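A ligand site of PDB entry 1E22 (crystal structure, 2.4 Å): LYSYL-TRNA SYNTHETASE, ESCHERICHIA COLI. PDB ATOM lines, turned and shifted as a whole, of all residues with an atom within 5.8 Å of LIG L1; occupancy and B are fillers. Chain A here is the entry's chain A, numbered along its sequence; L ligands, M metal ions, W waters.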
ATOM      1  N   GLY A 216      34.740 -26.720  31.486  1.00  0.00           N
ATOM      2  CA  GLY A 216      33.606 -27.544  31.132  1.00  0.00           C
ATOM      3  C   GLY A 216      32.447 -26.736  30.570  1.00  0.00           C
ATOM      4  O   GLY A 216      31.411 -27.286  30.180  1.00  0.00           O
ATOM      5  N   ALA A 217      32.616 -25.424  30.512  1.00  0.00           N
ATOM      6  CA  ALA A 217      31.591 -24.524  30.016  1.00  0.00           C
ATOM      7  C   ALA A 217      32.163 -23.127  29.935  1.00  0.00           C
ATOM      8  O   ALA A 217      33.304 -22.880  30.332  1.00  0.00           O
ATOM      9  CB  ALA A 217      30.375 -24.555  30.945  1.00  0.00           C
ATOM     10  N   ILE A 237      31.548 -24.301  37.328  1.00  0.00           N
ATOM     11  CA  ILE A 237      30.524 -23.889  36.382  1.00  0.00           C
ATOM     12  C   ILE A 237      30.015 -25.156  35.687  1.00  0.00           C
ATOM     13  O   ILE A 237      28.943 -25.151  35.089  1.00  0.00           O
ATOM     14  CB  ILE A 237      31.071 -22.889  35.345  1.00  0.00           C
ATOM     15  CG1 ILE A 237      32.185 -23.533  34.526  1.00  0.00           C
ATOM     16  CG2 ILE A 237      31.603 -21.637  36.050  1.00  0.00           C
ATOM     17  CD1 ILE A 237      32.843 -22.566  33.562  1.00  0.00           C
ATOM     18  N   ALA A 238      30.796 -26.234  35.787  1.00  0.00           N
ATOM     19  CA  ALA A 238      30.441 -27.525  35.197  1.00  0.00           C
ATOM     20  C   ALA A 238      31.393 -28.606  35.673  1.00  0.00           C
ATOM     21  O   ALA A 238      32.564 -28.347  35.885  1.00  0.00           O
ATOM     22  CB  ALA A 238      30.494 -27.443  33.683  1.00  0.00           C
ATOM     23  N   PRO A 239      30.890 -29.835  35.875  1.00  0.00           N
ATOM     24  CA  PRO A 239      31.725 -30.956  36.323  1.00  0.00           C
ATOM     25  C   PRO A 239      32.363 -31.731  35.175  1.00  0.00           C
ATOM     26  O   PRO A 239      33.137 -32.660  35.393  1.00  0.00           O
ATOM     27  CB  PRO A 239      30.740 -31.831  37.096  1.00  0.00           C
ATOM     28  CG  PRO A 239      29.462 -31.660  36.349  1.00  0.00           C
ATOM     29  CD  PRO A 239      29.474 -30.247  35.747  1.00  0.00           C
ATOM     30  N   GLU A 240      32.068 -31.340  33.935  1.00  0.00           N
ATOM     31  CA  GLU A 240      32.575 -32.024  32.758  1.00  0.00           C
ATOM     32  C   GLU A 240      34.014 -32.573  32.758  1.00  0.00           C
ATOM     33  O   GLU A 240      34.233 -33.770  32.539  1.00  0.00           O
ATOM     34  CB  GLU A 240      32.392 -31.161  31.511  1.00  0.00           C
ATOM     35  CG  GLU A 240      32.923 -31.826  30.252  1.00  0.00           C
ATOM     36  CD  GLU A 240      32.332 -31.267  28.976  1.00  0.00           C
ATOM     37  OE1 GLU A 240      31.292 -30.592  29.046  1.00  0.00           O
ATOM     38  OE2 GLU A 240      32.920 -31.506  27.901  1.00  0.00           O
ATOM     39  N   LYS A 244      34.907 -36.719  32.814  1.00  0.00           N
ATOM     40  CA  LYS A 244      35.575 -37.432  31.746  1.00  0.00           C
ATOM     41  C   LYS A 244      36.877 -38.063  32.228  1.00  0.00           C
ATOM     42  O   LYS A 244      37.336 -39.046  31.662  1.00  0.00           O
ATOM     43  CB  LYS A 244      35.807 -36.505  30.561  1.00  0.00           C
ATOM     44  CG  LYS A 244      34.710 -36.623  29.507  1.00  0.00           C
ATOM     45  CD  LYS A 244      35.012 -35.763  28.297  1.00  0.00           C
ATOM     46  CE  LYS A 244      34.710 -34.304  28.573  1.00  0.00           C
ATOM     47  NZ  LYS A 244      34.773 -33.548  27.310  1.00  0.00           N
ATOM     48  N   ASN A 260      25.696 -26.096  39.801  1.00  0.00           N
ATOM     49  CA  ASN A 260      26.705 -25.449  39.007  1.00  0.00           C
ATOM     50  C   ASN A 260      26.496 -24.026  39.475  1.00  0.00           C
ATOM     51  O   ASN A 260      25.408 -23.686  39.942  1.00  0.00           O
ATOM     52  CB  ASN A 260      26.400 -25.593  37.523  1.00  0.00           C
ATOM     53  CG  ASN A 260      26.961 -26.863  36.965  1.00  0.00           C
ATOM     54  OD1 ASN A 260      27.745 -27.542  37.629  1.00  0.00           O
ATOM     55  ND2 ASN A 260      26.581 -27.191  35.734  1.00  0.00           N
ATOM     56  N   ARG A 262      27.066 -19.998  38.300  1.00  0.00           N
ATOM     57  CA  ARG A 262      27.488 -19.099  37.249  1.00  0.00           C
ATOM     58  C   ARG A 262      27.193 -17.678  37.702  1.00  0.00           C
ATOM     59  O   ARG A 262      26.075 -17.336  38.072  1.00  0.00           O
ATOM     60  CB  ARG A 262      26.799 -19.479  35.942  1.00  0.00           C
ATOM     61  CG  ARG A 262      27.088 -20.949  35.625  1.00  0.00           C
ATOM     62  CD  ARG A 262      26.853 -21.337  34.192  1.00  0.00           C
ATOM     63  NE  ARG A 262      27.049 -22.779  34.030  1.00  0.00           N
ATOM     64  CZ  ARG A 262      27.010 -23.423  32.861  1.00  0.00           C
ATOM     65  NH1 ARG A 262      26.766 -22.759  31.736  1.00  0.00           N
ATOM     66  NH2 ARG A 262      27.217 -24.736  32.832  1.00  0.00           N
ATOM     67  N   MET A 276      22.161 -29.437  37.697  1.00  0.00           N
ATOM     68  CA  MET A 276      22.396 -30.003  36.386  1.00  0.00           C
ATOM     69  C   MET A 276      22.736 -31.473  36.485  1.00  0.00           C
ATOM     70  O   MET A 276      23.351 -31.919  37.456  1.00  0.00           O
ATOM     71  CB  MET A 276      23.541 -29.273  35.700  1.00  0.00           C
ATOM     72  CG  MET A 276      23.966 -29.948  34.431  1.00  0.00           C
ATOM     73  SD  MET A 276      24.124 -28.765  33.106  1.00  0.00           S
ATOM     74  CE  MET A 276      25.964 -28.613  33.088  1.00  0.00           C
ATOM     75  N   GLU A 278      24.840 -34.308  34.525  1.00  0.00           N
ATOM     76  CA  GLU A 278      25.783 -34.543  33.442  1.00  0.00           C
ATOM     77  C   GLU A 278      25.998 -36.060  33.436  1.00  0.00           C
ATOM     78  O   GLU A 278      26.170 -36.664  34.496  1.00  0.00           O
ATOM     79  CB  GLU A 278      27.103 -33.809  33.684  1.00  0.00           C
ATOM     80  CG  GLU A 278      27.086 -32.357  33.257  1.00  0.00           C
ATOM     81  CD  GLU A 278      28.438 -31.859  32.762  1.00  0.00           C
ATOM     82  OE1 GLU A 278      29.190 -32.665  32.181  1.00  0.00           O
ATOM     83  OE2 GLU A 278      28.738 -30.662  32.947  1.00  0.00           O
ATOM     84  N   TYR A 280      27.804 -39.485  31.134  1.00  0.00           N
ATOM     85  CA  TYR A 280      28.772 -39.866  30.120  1.00  0.00           C
ATOM     86  C   TYR A 280      28.702 -41.357  29.905  1.00  0.00           C
ATOM     87  O   TYR A 280      28.625 -42.110  30.870  1.00  0.00           O
ATOM     88  CB  TYR A 280      30.189 -39.470  30.554  1.00  0.00           C
ATOM     89  CG  TYR A 280      30.395 -37.965  30.554  1.00  0.00           C
ATOM     90  CD1 TYR A 280      29.954 -37.181  31.624  1.00  0.00           C
ATOM     91  CD2 TYR A 280      30.944 -37.327  29.436  1.00  0.00           C
ATOM     92  CE1 TYR A 280      30.028 -35.780  31.564  1.00  0.00           C
ATOM     93  CE2 TYR A 280      31.026 -35.936  29.371  1.00  0.00           C
ATOM     94  CZ  TYR A 280      30.565 -35.166  30.437  1.00  0.00           C
ATOM     95  OH  TYR A 280      30.620 -33.789  30.356  1.00  0.00           O
ATOM     96  N   ARG A 412      27.881 -31.902  18.126  1.00  0.00           N
ATOM     97  CA  ARG A 412      27.186 -31.383  19.279  1.00  0.00           C
ATOM     98  C   ARG A 412      25.773 -30.942  18.957  1.00  0.00           C
ATOM     99  O   ARG A 412      25.467 -30.564  17.832  1.00  0.00           O
ATOM    100  CB  ARG A 412      27.980 -30.206  19.843  1.00  0.00           C
ATOM    101  CG  ARG A 412      27.244 -29.455  20.919  1.00  0.00           C
ATOM    102  CD  ARG A 412      28.077 -28.323  21.443  1.00  0.00           C
ATOM    103  NE  ARG A 412      27.353 -27.567  22.446  1.00  0.00           N
ATOM    104  CZ  ARG A 412      27.590 -26.288  22.719  1.00  0.00           C
ATOM    105  NH1 ARG A 412      28.546 -25.654  22.049  1.00  0.00           N
ATOM    106  NH2 ARG A 412      26.885 -25.653  23.645  1.00  0.00           N
ATOM    107  N   GLU A 414      21.995 -29.239  21.109  1.00  0.00           N
ATOM    108  CA  GLU A 414      21.390 -28.689  22.307  1.00  0.00           C
ATOM    109  C   GLU A 414      19.931 -28.935  22.012  1.00  0.00           C
ATOM    110  O   GLU A 414      19.538 -29.001  20.853  1.00  0.00           O
ATOM    111  CB  GLU A 414      21.686 -27.198  22.426  1.00  0.00           C
ATOM    112  CG  GLU A 414      23.107 -26.911  22.834  1.00  0.00           C
ATOM    113  CD  GLU A 414      23.264 -25.552  23.501  1.00  0.00           C
ATOM    114  OE1 GLU A 414      22.739 -24.555  22.957  1.00  0.00           O
ATOM    115  OE2 GLU A 414      23.924 -25.476  24.572  1.00  0.00           O
ATOM    116  N   ASN A 424      22.338 -29.941  26.634  1.00  0.00           N
ATOM    117  CA  ASN A 424      23.486 -29.730  25.777  1.00  0.00           C
ATOM    118  C   ASN A 424      24.255 -31.044  25.812  1.00  0.00           C
ATOM    119  O   ASN A 424      24.674 -31.493  26.870  1.00  0.00           O
ATOM    120  CB  ASN A 424      24.322 -28.608  26.366  1.00  0.00           C
ATOM    121  CG  ASN A 424      25.602 -28.352  25.594  1.00  0.00           C
ATOM    122  OD1 ASN A 424      25.786 -28.811  24.462  1.00  0.00           O
ATOM    123  ND2 ASN A 424      26.492 -27.592  26.212  1.00  0.00           N
ATOM    124  N   GLY A 425      24.429 -31.672  24.654  1.00  0.00           N
ATOM    125  CA  GLY A 425      25.134 -32.931  24.603  1.00  0.00           C
ATOM    126  C   GLY A 425      25.967 -33.098  23.355  1.00  0.00           C
ATOM    127  O   GLY A 425      25.706 -32.455  22.348  1.00  0.00           O
ATOM    128  N   PHE A 426      27.004 -33.927  23.428  1.00  0.00           N
ATOM    129  CA  PHE A 426      27.842 -34.186  22.261  1.00  0.00           C
ATOM    130  C   PHE A 426      28.791 -35.380  22.358  1.00  0.00           C
ATOM    131  O   PHE A 426      28.944 -35.997  23.414  1.00  0.00           O
ATOM    132  CB  PHE A 426      28.666 -32.937  21.896  1.00  0.00           C
ATOM    133  CG  PHE A 426      29.335 -32.267  23.079  1.00  0.00           C
ATOM    134  CD1 PHE A 426      30.561 -32.725  23.555  1.00  0.00           C
ATOM    135  CD2 PHE A 426      28.774 -31.126  23.647  1.00  0.00           C
ATOM    136  CE1 PHE A 426      31.220 -32.054  24.596  1.00  0.00           C
ATOM    137  CE2 PHE A 426      29.425 -30.444  24.693  1.00  0.00           C
ATOM    138  CZ  PHE A 426      30.659 -30.913  25.164  1.00  0.00           C
ATOM    139  N   GLU A 428      32.124 -36.638  22.789  1.00  0.00           N
ATOM    140  CA  GLU A 428      33.272 -36.022  23.450  1.00  0.00           C
ATOM    141  C   GLU A 428      34.527 -36.004  22.613  1.00  0.00           C
ATOM    142  O   GLU A 428      34.743 -36.900  21.780  1.00  0.00           O
ATOM    143  CB  GLU A 428      33.539 -36.728  24.768  1.00  0.00           C
ATOM    144  CG  GLU A 428      32.336 -36.756  25.672  1.00  0.00           C
ATOM    145  CD  GLU A 428      31.835 -35.356  25.987  1.00  0.00           C
ATOM    146  OE1 GLU A 428      32.655 -34.403  25.925  1.00  0.00           O
ATOM    147  OE2 GLU A 428      30.629 -35.206  26.295  1.00  0.00           O
ATOM    148  N   GLY A 473      28.509 -37.345  26.034  1.00  0.00           N
ATOM    149  CA  GLY A 473      28.107 -36.753  27.297  1.00  0.00           C
ATOM    150  C   GLY A 473      26.902 -35.849  27.109  1.00  0.00           C
ATOM    151  O   GLY A 473      26.742 -35.222  26.058  1.00  0.00           O
ATOM    152  N   LEU A 474      26.058 -35.746  28.126  1.00  0.00           N
ATOM    153  CA  LEU A 474      24.870 -34.921  28.036  1.00  0.00           C
ATOM    154  C   LEU A 474      24.700 -34.101  29.297  1.00  0.00           C
ATOM    155  O   LEU A 474      24.973 -34.585  30.394  1.00  0.00           O
ATOM    156  CB  LEU A 474      23.641 -35.821  27.832  1.00  0.00           C
ATOM    157  CG  LEU A 474      22.255 -35.196  27.716  1.00  0.00           C
ATOM    158  CD1 LEU A 474      22.177 -34.316  26.463  1.00  0.00           C
ATOM    159  CD2 LEU A 474      21.215 -36.306  27.664  1.00  0.00           C
ATOM    160  N   GLY A 475      24.249 -32.867  29.128  1.00  0.00           N
ATOM    161  CA  GLY A 475      24.034 -31.992  30.258  1.00  0.00           C
ATOM    162  C   GLY A 475      22.616 -31.459  30.163  1.00  0.00           C
ATOM    163  O   GLY A 475      22.257 -30.822  29.191  1.00  0.00           O
HETATM  164  N1  LIG L   1      29.317 -29.161  30.569  1.00  0.00           N
HETATM  165  C1  LIG L   1      28.248 -28.852  29.627  1.00  0.00           C
HETATM  166  C2  LIG L   1      27.635 -27.480  29.918  1.00  0.00           C
HETATM  167  O1  LIG L   1      27.783 -26.998  31.064  1.00  0.00           O
HETATM  168  C3  LIG L   1      27.164 -29.931  29.684  1.00  0.00           C
HETATM  169  C4  LIG L   1      27.615 -31.293  29.201  1.00  0.00           C
HETATM  170  C5  LIG L   1      28.232 -31.198  27.825  1.00  0.00           C
HETATM  171  C6  LIG L   1      28.456 -32.582  27.215  1.00  0.00           C
HETATM  172  N2  LIG L   1      29.838 -33.076  27.473  1.00  0.00           N
HETATM  173  O2  LIG L   1      27.014 -26.909  28.999  1.00  0.00           O
HETATM  174  P1  LG2 L   2      20.932 -20.074  28.152  1.00  0.00           P
HETATM  175  O1  LG2 L   2      21.580 -18.855  28.730  1.00  0.00           O
HETATM  176  O2  LG2 L   2      19.502 -20.261  28.543  1.00  0.00           O
HETATM  177  O3  LG2 L   2      21.188 -20.269  26.692  1.00  0.00           O
HETATM  178  P2  LG2 L   2      23.588 -21.667  28.476  1.00  0.00           P
HETATM  179  O4  LG2 L   2      23.656 -22.093  27.057  1.00  0.00           O
HETATM  180  O5  LG2 L   2      24.310 -20.445  28.926  1.00  0.00           O
HETATM  181  C1  LG2 L   2      21.788 -21.510  28.988  1.00  0.00           C
HETATM  182  P3  LG2 L   2      24.983 -24.141  28.937  1.00  0.00           P
HETATM  183  O6  LG2 L   2      24.459 -24.722  27.681  1.00  0.00           O
HETATM  184  O7  LG2 L   2      26.399 -23.682  28.966  1.00  0.00           O
HETATM  185  O8  LG2 L   2      24.067 -22.898  29.389  1.00  0.00           O
HETATM  186  O9  LG2 L   2      24.698 -25.162  30.130  1.00  0.00           O
HETATM  187  C2  LG2 L   2      23.918 -26.339  29.921  1.00  0.00           C
HETATM  188  C3  LG2 L   2      22.518 -26.184  30.489  1.00  0.00           C
HETATM  189  O10 LG2 L   2      22.522 -25.641  31.838  1.00  0.00           O
HETATM  190  C4  LG2 L   2      21.585 -25.266  29.738  1.00  0.00           C
HETATM  191  O11 LG2 L   2      21.056 -25.966  28.628  1.00  0.00           O
HETATM  192  C5  LG2 L   2      20.489 -25.005  30.773  1.00  0.00           C
HETATM  193  O12 LG2 L   2      19.622 -26.114  30.848  1.00  0.00           O
HETATM  194  C6  LG2 L   2      21.313 -24.947  32.076  1.00  0.00           C
HETATM  195  N1  LG2 L   2      21.610 -23.603  32.560  1.00  0.00           N
HETATM  196  C7  LG2 L   2      22.636 -22.768  32.168  1.00  0.00           C
HETATM  197  N2  LG2 L   2      22.699 -21.653  32.854  1.00  0.00           N
HETATM  198  C8  LG2 L   2      21.644 -21.740  33.744  1.00  0.00           C
HETATM  199  C9  LG2 L   2      21.187 -20.883  34.732  1.00  0.00           C
HETATM  200  N3  LG2 L   2      21.786 -19.731  35.043  1.00  0.00           N
HETATM  201  N4  LG2 L   2      20.082 -21.256  35.432  1.00  0.00           N
HETATM  202  C10 LG2 L   2      19.498 -22.419  35.129  1.00  0.00           C
HETATM  203  N5  LG2 L   2      19.850 -23.332  34.230  1.00  0.00           N
HETATM  204  C11 LG2 L   2      20.952 -22.926  33.556  1.00  0.00           C
HETATM  205 MG    MG M   1      24.905 -23.688  25.720  1.00  0.00          MG
HETATM  206  O   HOH W   1      31.219 -28.105  27.872  1.00  0.00           O
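OE2 of Glu 428 is in salt-bridge range of N2 of LIG L1 (2.6 Å).
N1 of LIG L1 sits at hydrogen-bond distance from O of Gly 216 (2.8 Å).
N1 of LIG L1 is in salt-bridge range of OE2 of Glu 278 (2.9 Å).
N1 of LIG L1 is in salt-bridge range of OE1 of Glu 240 (2.9 Å).
An oxygen (O2) of LIG L1 lies within hydrogen-bond range of the side-chain amide nitrogen (ND2) of Asn 424, at 2.9 Å.
O1 of LIG L1 lies within salt-bridge range of NH2 of Arg 262 (2.9 Å).
The side-chain hydroxyl (OH) of Tyr 280 sits at hydrogen-bond distance from a nitrogen (N2) of LIG L1, 3.1 Å away.
The guanidinium group of Arg 262 is in salt-bridge range of an oxygen (O7) of LG2 L2.
N of Gly 473 lies within hydrogen-bond range of OE2 of Glu 428, at 3.0 Å.
The side-chain carboxylate of Glu 428 lies within salt-bridge range of the side-chain amino group of Lys 244, 2.7 Å away.
The side-chain carboxylate (OE1) of Glu 278 sits at hydrogen-bond distance from the side-chain hydroxyl (OH) of Tyr 280 (2.6 Å).
The side-chain carboxylate (OE2) of Glu 240 lies within salt-bridge range of the side-chain amino group (NZ) of Lys 244, 2.8 Å away.
The backbone carbonyl oxygen (O) of Asn 424 lies within hydrogen-bond range of the backbone NH (N) of Gly 475 (2.7 Å).
The side-chain amide oxygen of Asn 424 is in hydrogen-bond range of the guanidinium group of Arg 412.
The backbone carbonyl oxygen (O) of Ile 237 sits at hydrogen-bond distance from the guanidinium group (NH2) of Arg 262 (2.9 Å).
O of Gly 473 lies within hydrogen-bond range of N of Phe 426, at 2.9 Å.
Residues that only touch LIG L1: Met 276 (3.2 Å), Phe 426 (3.3 Å), Gly 473 (3.4 Å), Ala 217 (3.6 Å), Gly 475 (3.7 Å) and Ala 238 (3.7 Å).
Of the 21 residues printed, 13 come within 4 Å of LIG L1.
Along chain A the residues within 4 Å of LIG L1 span positions 216 to 475.
The nearest printed residue that does not touch LIG L1 is Leu 474 (4.05 Å).
Water W1 lies within hydrogen-bond range of O of Gly 216 (2.5 Å), OE1 of Glu 240 (2.8 Å) and N1 of LIG L1 (3.5 Å).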
